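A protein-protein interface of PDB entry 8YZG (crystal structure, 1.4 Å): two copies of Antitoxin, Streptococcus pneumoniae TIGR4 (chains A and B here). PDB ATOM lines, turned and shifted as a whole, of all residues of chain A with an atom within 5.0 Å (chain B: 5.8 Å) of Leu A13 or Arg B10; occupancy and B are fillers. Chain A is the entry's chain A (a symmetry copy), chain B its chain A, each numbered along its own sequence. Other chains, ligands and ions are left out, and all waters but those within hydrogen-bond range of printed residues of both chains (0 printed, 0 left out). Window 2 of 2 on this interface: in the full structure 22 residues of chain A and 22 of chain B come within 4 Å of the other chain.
Leu B13 touches Arg A10 (CD2 to CB, 3.9 Å).
Leu A13 touches Tyr B6 (CD2 to CE1, 3.6 Å).
Leu A13 touches Arg B10 (CD2 to CB, 3.9 Å).
CG of Lys A14 touches OH of Tyr B6 (3.4 Å).
Tyr B6 touches Met A17 (CE1 to SD, 3.6 Å).
CE of Met A17 touches CE2 of Phe B9, 3.8 Å away.
Met A17 touches Ile B38.
The guanidinium group (NH2) of Arg B10 sits at hydrogen-bond distance from the side-chain amide oxygen (OD1) of Asn B11, at 3.1 Å.
The guanidinium group (NH2) of Arg A10 lies within hydrogen-bond range of the side-chain amide oxygen (OD1) of Asn A11, 3.1 Å away.
Leu A13 touches two residues of chain B.
Of chain A, only Leu A13 comes within 4 Å of Arg B10.
Printed residues of chain A within 4 Å of Tyr B6: Leu A13 (3.6 Å), Lys A14 (3.4 Å) and Met A17 (3.6 Å).
Of the printed residues of chain B, Arg A10 touches Leu B13.
The nearest residue of chain B that does not touch Leu A13 is Phe B9 (4.3 Å).
The nearest printed residue of chain A that does not touch Arg B10 is Lys A14 (5.8 Å).
Arg A10 touches Leu B13, and with the chains exchanged Leu A13 touches Arg B10.
Printed residues of chain A that touch a printed residue of chain B: Arg A10, Leu A13, Lys A14 and Met A17.
Among the printed residues, 7 pairs touch across the chains.
Among the printed residues, no Asp or Glu carboxylate lies within 4 Å of a Lys or Arg side-chain nitrogen of the other chain.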
ATOM      1  N   PHE A   9       0.523 -15.964  24.691  1.00  0.00           N
ATOM      2  CA  PHE A   9       0.604 -14.611  24.153  1.00  0.00           C
ATOM      3  C   PHE A   9      -0.297 -14.448  22.927  1.00  0.00           C
ATOM      4  O   PHE A   9      -1.102 -13.511  22.852  1.00  0.00           O
ATOM      5  CB  PHE A   9       2.071 -14.326  23.824  1.00  0.00           C
ATOM      6  CG  PHE A   9       2.318 -12.957  23.260  1.00  0.00           C
ATOM      7  CD1 PHE A   9       2.166 -11.825  24.043  1.00  0.00           C
ATOM      8  CD2 PHE A   9       2.698 -12.802  21.937  1.00  0.00           C
ATOM      9  CE1 PHE A   9       2.394 -10.546  23.515  1.00  0.00           C
ATOM     10  CE2 PHE A   9       2.944 -11.533  21.413  1.00  0.00           C
ATOM     11  CZ  PHE A   9       2.780 -10.415  22.196  1.00  0.00           C
ATOM     12  N   ARG A  10      -0.188 -15.371  21.967  1.00  0.00           N
ATOM     13  CA  ARG A  10      -1.015 -15.313  20.766  1.00  0.00           C
ATOM     14  C   ARG A  10      -2.499 -15.357  21.111  1.00  0.00           C
ATOM     15  O   ARG A  10      -3.299 -14.610  20.540  1.00  0.00           O
ATOM     16  CB  ARG A  10      -0.627 -16.471  19.843  1.00  0.00           C
ATOM     17  CG  ARG A  10      -1.427 -16.572  18.563  1.00  0.00           C
ATOM     18  CD  ARG A  10      -1.457 -18.010  18.077  1.00  0.00           C
ATOM     19  NE  ARG A  10      -1.990 -18.895  19.108  1.00  0.00           N
ATOM     20  CZ  ARG A  10      -1.620 -20.159  19.279  1.00  0.00           C
ATOM     21  NH1 ARG A  10      -0.711 -20.702  18.480  1.00  0.00           N
ATOM     22  NH2 ARG A  10      -2.162 -20.880  20.254  1.00  0.00           N
ATOM     23  N   ASN A  11      -2.875 -16.198  22.077  1.00  0.00           N
ATOM     24  CA  ASN A  11      -4.281 -16.385  22.425  1.00  0.00           C
ATOM     25  C   ASN A  11      -4.867 -15.201  23.169  1.00  0.00           C
ATOM     26  O   ASN A  11      -6.091 -15.116  23.305  1.00  0.00           O
ATOM     27  CB  ASN A  11      -4.453 -17.589  23.355  1.00  0.00           C
ATOM     28  CG  ASN A  11      -4.208 -18.893  22.669  1.00  0.00           C
ATOM     29  OD1 ASN A  11      -4.248 -18.977  21.444  1.00  0.00           O
ATOM     30  ND2 ASN A  11      -3.953 -19.939  23.460  1.00  0.00           N
ATOM     31  N   HIS A  12      -4.032 -14.314  23.700  1.00  0.00           N
ATOM     32  CA  HIS A  12      -4.502 -13.203  24.519  1.00  0.00           C
ATOM     33  C   HIS A  12      -3.763 -11.931  24.152  1.00  0.00           C
ATOM     34  O   HIS A  12      -3.412 -11.124  25.016  1.00  0.00           O
ATOM     35  CB  HIS A  12      -4.344 -13.517  26.005  1.00  0.00           C
ATOM     36  CG  HIS A  12      -5.033 -14.779  26.409  1.00  0.00           C
ATOM     37  ND1 HIS A  12      -6.389 -14.834  26.656  1.00  0.00           N
ATOM     38  CD2 HIS A  12      -4.566 -16.037  26.567  1.00  0.00           C
ATOM     39  CE1 HIS A  12      -6.723 -16.074  26.962  1.00  0.00           C
ATOM     40  NE2 HIS A  12      -5.638 -16.823  26.919  1.00  0.00           N
ATOM     41  N   LEU A  13      -3.571 -11.714  22.852  1.00  0.00           N
ATOM     42  CA  LEU A  13      -2.670 -10.665  22.386  1.00  0.00           C
ATOM     43  C   LEU A  13      -3.107  -9.287  22.870  1.00  0.00           C
ATOM     44  O   LEU A  13      -2.300  -8.530  23.426  1.00  0.00           O
ATOM     45  CB  LEU A  13      -2.614 -10.701  20.865  1.00  0.00           C
ATOM     46  CG  LEU A  13      -1.617  -9.772  20.193  1.00  0.00           C
ATOM     47  CD1 LEU A  13      -0.245 -10.075  20.727  1.00  0.00           C
ATOM     48  CD2 LEU A  13      -1.659  -9.959  18.686  1.00  0.00           C
ATOM     49  N   LYS A  14      -4.386  -8.944  22.689  1.00  0.00           N
ATOM     50  CA  LYS A  14      -4.857  -7.630  23.108  1.00  0.00           C
ATOM     51  C   LYS A  14      -4.719  -7.447  24.613  1.00  0.00           C
ATOM     52  O   LYS A  14      -4.330  -6.370  25.080  1.00  0.00           O
ATOM     53  CB  LYS A  14      -6.303  -7.401  22.666  1.00  0.00           C
ATOM     54  CG  LYS A  14      -6.473  -7.170  21.168  1.00  0.00           C
ATOM     55  CD  LYS A  14      -7.895  -6.733  20.836  1.00  0.00           C
ATOM     56  CE  LYS A  14      -8.193  -6.888  19.357  1.00  0.00           C
ATOM     57  NZ  LYS A  14      -9.628  -6.605  19.060  1.00  0.00           N
ATOM     58  N   ASP A  15      -5.032  -8.484  25.395  1.00  0.00           N
ATOM     59  CA  ASP A  15      -4.871  -8.375  26.843  1.00  0.00           C
ATOM     60  C   ASP A  15      -3.426  -8.066  27.222  1.00  0.00           C
ATOM     61  O   ASP A  15      -3.170  -7.251  28.118  1.00  0.00           O
ATOM     62  CB  ASP A  15      -5.324  -9.660  27.546  1.00  0.00           C
ATOM     63  CG  ASP A  15      -6.836  -9.825  27.592  1.00  0.00           C
ATOM     64  OD1 ASP A  15      -7.567  -8.847  27.341  1.00  0.00           O
ATOM     65  OD2 ASP A  15      -7.282 -10.953  27.892  1.00  0.00           O
ATOM     66  N   TYR A  16      -2.465  -8.721  26.576  1.00  0.00           N
ATOM     67  CA  TYR A  16      -1.068  -8.465  26.909  1.00  0.00           C
ATOM     68  C   TYR A  16      -0.612  -7.084  26.454  1.00  0.00           C
ATOM     69  O   TYR A  16       0.210  -6.448  27.129  1.00  0.00           O
ATOM     70  CB  TYR A  16      -0.182  -9.586  26.381  1.00  0.00           C
ATOM     71  CG  TYR A  16      -0.236 -10.819  27.250  1.00  0.00           C
ATOM     72  CD1 TYR A  16       0.207 -10.782  28.579  1.00  0.00           C
ATOM     73  CD2 TYR A  16      -0.730 -12.013  26.755  1.00  0.00           C
ATOM     74  CE1 TYR A  16       0.163 -11.912  29.391  1.00  0.00           C
ATOM     75  CE2 TYR A  16      -0.773 -13.143  27.546  1.00  0.00           C
ATOM     76  CZ  TYR A  16      -0.343 -13.087  28.858  1.00  0.00           C
ATOM     77  OH  TYR A  16      -0.374 -14.241  29.607  1.00  0.00           O
ATOM     78  N   MET A  17      -1.103  -6.614  25.309  1.00  0.00           N
ATOM     79  CA  MET A  17      -0.792  -5.253  24.887  1.00  0.00           C
ATOM     80  C   MET A  17      -1.320  -4.237  25.888  1.00  0.00           C
ATOM     81  O   MET A  17      -0.622  -3.274  26.232  1.00  0.00           O
ATOM     82  CB  MET A  17      -1.360  -5.010  23.496  1.00  0.00           C
ATOM     83  CG  MET A  17      -0.673  -5.862  22.431  1.00  0.00           C
ATOM     84  SD  MET A  17      -1.391  -5.602  20.806  1.00  0.00           S
ATOM     85  CE  MET A  17      -0.191  -6.395  19.745  1.00  0.00           C
ATOM     86  N   LEU B   5       0.582  -2.365  11.479  1.00  0.00           N
ATOM     87  CA  LEU B   5      -0.789  -2.337  11.980  1.00  0.00           C
ATOM     88  C   LEU B   5      -1.088  -3.573  12.819  1.00  0.00           C
ATOM     89  O   LEU B   5      -0.640  -4.679  12.511  1.00  0.00           O
ATOM     90  CB  LEU B   5      -1.765  -2.296  10.804  1.00  0.00           C
ATOM     91  CG  LEU B   5      -1.682  -1.010   9.981  1.00  0.00           C
ATOM     92  CD1 LEU B   5      -2.457  -1.170   8.685  1.00  0.00           C
ATOM     93  CD2 LEU B   5      -2.180   0.184  10.771  1.00  0.00           C
ATOM     94  N   TYR B   6      -1.888  -3.380  13.873  1.00  0.00           N
ATOM     95  CA  TYR B   6      -2.255  -4.492  14.743  1.00  0.00           C
ATOM     96  C   TYR B   6      -2.713  -5.723  13.960  1.00  0.00           C
ATOM     97  O   TYR B   6      -2.248  -6.838  14.213  1.00  0.00           O
ATOM     98  CB  TYR B   6      -3.354  -4.070  15.724  1.00  0.00           C
ATOM     99  CG  TYR B   6      -3.851  -5.278  16.484  1.00  0.00           C
ATOM    100  CD1 TYR B   6      -3.095  -5.832  17.515  1.00  0.00           C
ATOM    101  CD2 TYR B   6      -5.030  -5.919  16.117  1.00  0.00           C
ATOM    102  CE1 TYR B   6      -3.525  -6.971  18.181  1.00  0.00           C
ATOM    103  CE2 TYR B   6      -5.458  -7.057  16.773  1.00  0.00           C
ATOM    104  CZ  TYR B   6      -4.700  -7.578  17.802  1.00  0.00           C
ATOM    105  OH  TYR B   6      -5.126  -8.709  18.470  1.00  0.00           O
ATOM    106  N   SER B   7      -3.659  -5.552  13.033  1.00  0.00           N
ATOM    107  CA  SER B   7      -4.194  -6.724  12.341  1.00  0.00           C
ATOM    108  C   SER B   7      -3.105  -7.452  11.560  1.00  0.00           C
ATOM    109  O   SER B   7      -3.064  -8.689  11.530  1.00  0.00           O
ATOM    110  CB  SER B   7      -5.350  -6.324  11.423  1.00  0.00           C
ATOM    111  OG  SER B   7      -4.980  -5.298  10.526  1.00  0.00           O
ATOM    112  N   THR B   8      -2.199  -6.698  10.944  1.00  0.00           N
ATOM    113  CA  THR B   8      -1.114  -7.312  10.188  1.00  0.00           C
ATOM    114  C   THR B   8      -0.154  -8.055  11.106  1.00  0.00           C
ATOM    115  O   THR B   8       0.294  -9.164  10.789  1.00  0.00           O
ATOM    116  CB  THR B   8      -0.398  -6.236   9.388  1.00  0.00           C
ATOM    117  OG1 THR B   8      -1.356  -5.608   8.523  1.00  0.00           O
ATOM    118  CG2 THR B   8       0.723  -6.825   8.567  1.00  0.00           C
ATOM    119  N   PHE B   9       0.170  -7.449  12.247  1.00  0.00           N
ATOM    120  CA  PHE B   9       1.018  -8.099  13.240  1.00  0.00           C
ATOM    121  C   PHE B   9       0.400  -9.413  13.722  1.00  0.00           C
ATOM    122  O   PHE B   9       1.059 -10.460  13.725  1.00  0.00           O
ATOM    123  CB  PHE B   9       1.230  -7.113  14.390  1.00  0.00           C
ATOM    124  CG  PHE B   9       2.093  -7.640  15.499  1.00  0.00           C
ATOM    125  CD1 PHE B   9       3.446  -7.862  15.305  1.00  0.00           C
ATOM    126  CD2 PHE B   9       1.547  -7.921  16.741  1.00  0.00           C
ATOM    127  CE1 PHE B   9       4.253  -8.358  16.339  1.00  0.00           C
ATOM    128  CE2 PHE B   9       2.350  -8.397  17.778  1.00  0.00           C
ATOM    129  CZ  PHE B   9       3.689  -8.624  17.571  1.00  0.00           C
ATOM    130  N   ARG B  10      -0.879  -9.375  14.108  1.00  0.00           N
ATOM    131  CA  ARG B  10      -1.565 -10.579  14.569  1.00  0.00           C
ATOM    132  C   ARG B  10      -1.566 -11.661  13.495  1.00  0.00           C
ATOM    133  O   ARG B  10      -1.334 -12.837  13.789  1.00  0.00           O
ATOM    134  CB  ARG B  10      -2.990 -10.207  14.983  1.00  0.00           C
ATOM    135  CG  ARG B  10      -3.848 -11.362  15.451  1.00  0.00           C
ATOM    136  CD  ARG B  10      -5.315 -11.058  15.203  1.00  0.00           C
ATOM    137  NE  ARG B  10      -5.552 -10.756  13.795  1.00  0.00           N
ATOM    138  CZ  ARG B  10      -6.478  -9.912  13.352  1.00  0.00           C
ATOM    139  NH1 ARG B  10      -7.269  -9.280  14.209  1.00  0.00           N
ATOM    140  NH2 ARG B  10      -6.609  -9.701  12.047  1.00  0.00           N
ATOM    141  N   ASN B  11      -1.786 -11.271  12.237  1.00  0.00           N
ATOM    142  CA  ASN B  11      -1.898 -12.234  11.145  1.00  0.00           C
ATOM    143  C   ASN B  11      -0.568 -12.855  10.766  1.00  0.00           C
ATOM    144  O   ASN B  11      -0.549 -13.852  10.039  1.00  0.00           O
ATOM    145  CB  ASN B  11      -2.420 -11.555   9.876  1.00  0.00           C
ATOM    146  CG  ASN B  11      -3.854 -11.151   9.979  1.00  0.00           C
ATOM    147  OD1 ASN B  11      -4.590 -11.656  10.824  1.00  0.00           O
ATOM    148  ND2 ASN B  11      -4.274 -10.231   9.107  1.00  0.00           N
ATOM    149  N   HIS B  12       0.545 -12.265  11.190  1.00  0.00           N
ATOM    150  CA  HIS B  12       1.867 -12.731  10.788  1.00  0.00           C
ATOM    151  C   HIS B  12       2.808 -12.731  11.978  1.00  0.00           C
ATOM    152  O   HIS B  12       3.984 -12.381  11.863  1.00  0.00           O
ATOM    153  CB  HIS B  12       2.424 -11.875   9.653  1.00  0.00           C
ATOM    154  CG  HIS B  12       1.518 -11.822   8.467  1.00  0.00           C
ATOM    155  ND1 HIS B  12       1.466 -12.833   7.530  1.00  0.00           N
ATOM    156  CD2 HIS B  12       0.600 -10.905   8.088  1.00  0.00           C
ATOM    157  CE1 HIS B  12       0.561 -12.531   6.618  1.00  0.00           C
ATOM    158  NE2 HIS B  12       0.024 -11.368   6.929  1.00  0.00           N
ATOM    159  N   LEU B  13       2.306 -13.182  13.127  1.00  0.00           N
ATOM    160  CA  LEU B  13       3.023 -13.005  14.385  1.00  0.00           C
ATOM    161  C   LEU B  13       4.391 -13.679  14.357  1.00  0.00           C
ATOM    162  O   LEU B  13       5.406 -13.055  14.694  1.00  0.00           O
ATOM    163  CB  LEU B  13       2.177 -13.568  15.519  1.00  0.00           C
ATOM    164  CG  LEU B  13       2.692 -13.352  16.931  1.00  0.00           C
ATOM    165  CD1 LEU B  13       2.869 -11.876  17.157  1.00  0.00           C
ATOM    166  CD2 LEU B  13       1.717 -13.935  17.941  1.00  0.00           C
ATOM    167  N   ILE B  38       2.536  -0.827  21.127  1.00  0.00           N
ATOM    168  CA  ILE B  38       3.642  -1.559  21.715  1.00  0.00           C
ATOM    169  C   ILE B  38       4.851  -1.486  20.808  1.00  0.00           C
ATOM    170  O   ILE B  38       4.773  -1.123  19.629  1.00  0.00           O
ATOM    171  CB  ILE B  38       3.318  -3.037  22.039  1.00  0.00           C
ATOM    172  CG1 ILE B  38       2.932  -3.803  20.775  1.00  0.00           C
ATOM    173  CG2 ILE B  38       2.227  -3.151  23.095  1.00  0.00           C
ATOM    174  CD1 ILE B  38       2.995  -5.311  20.933  1.00  0.00           C
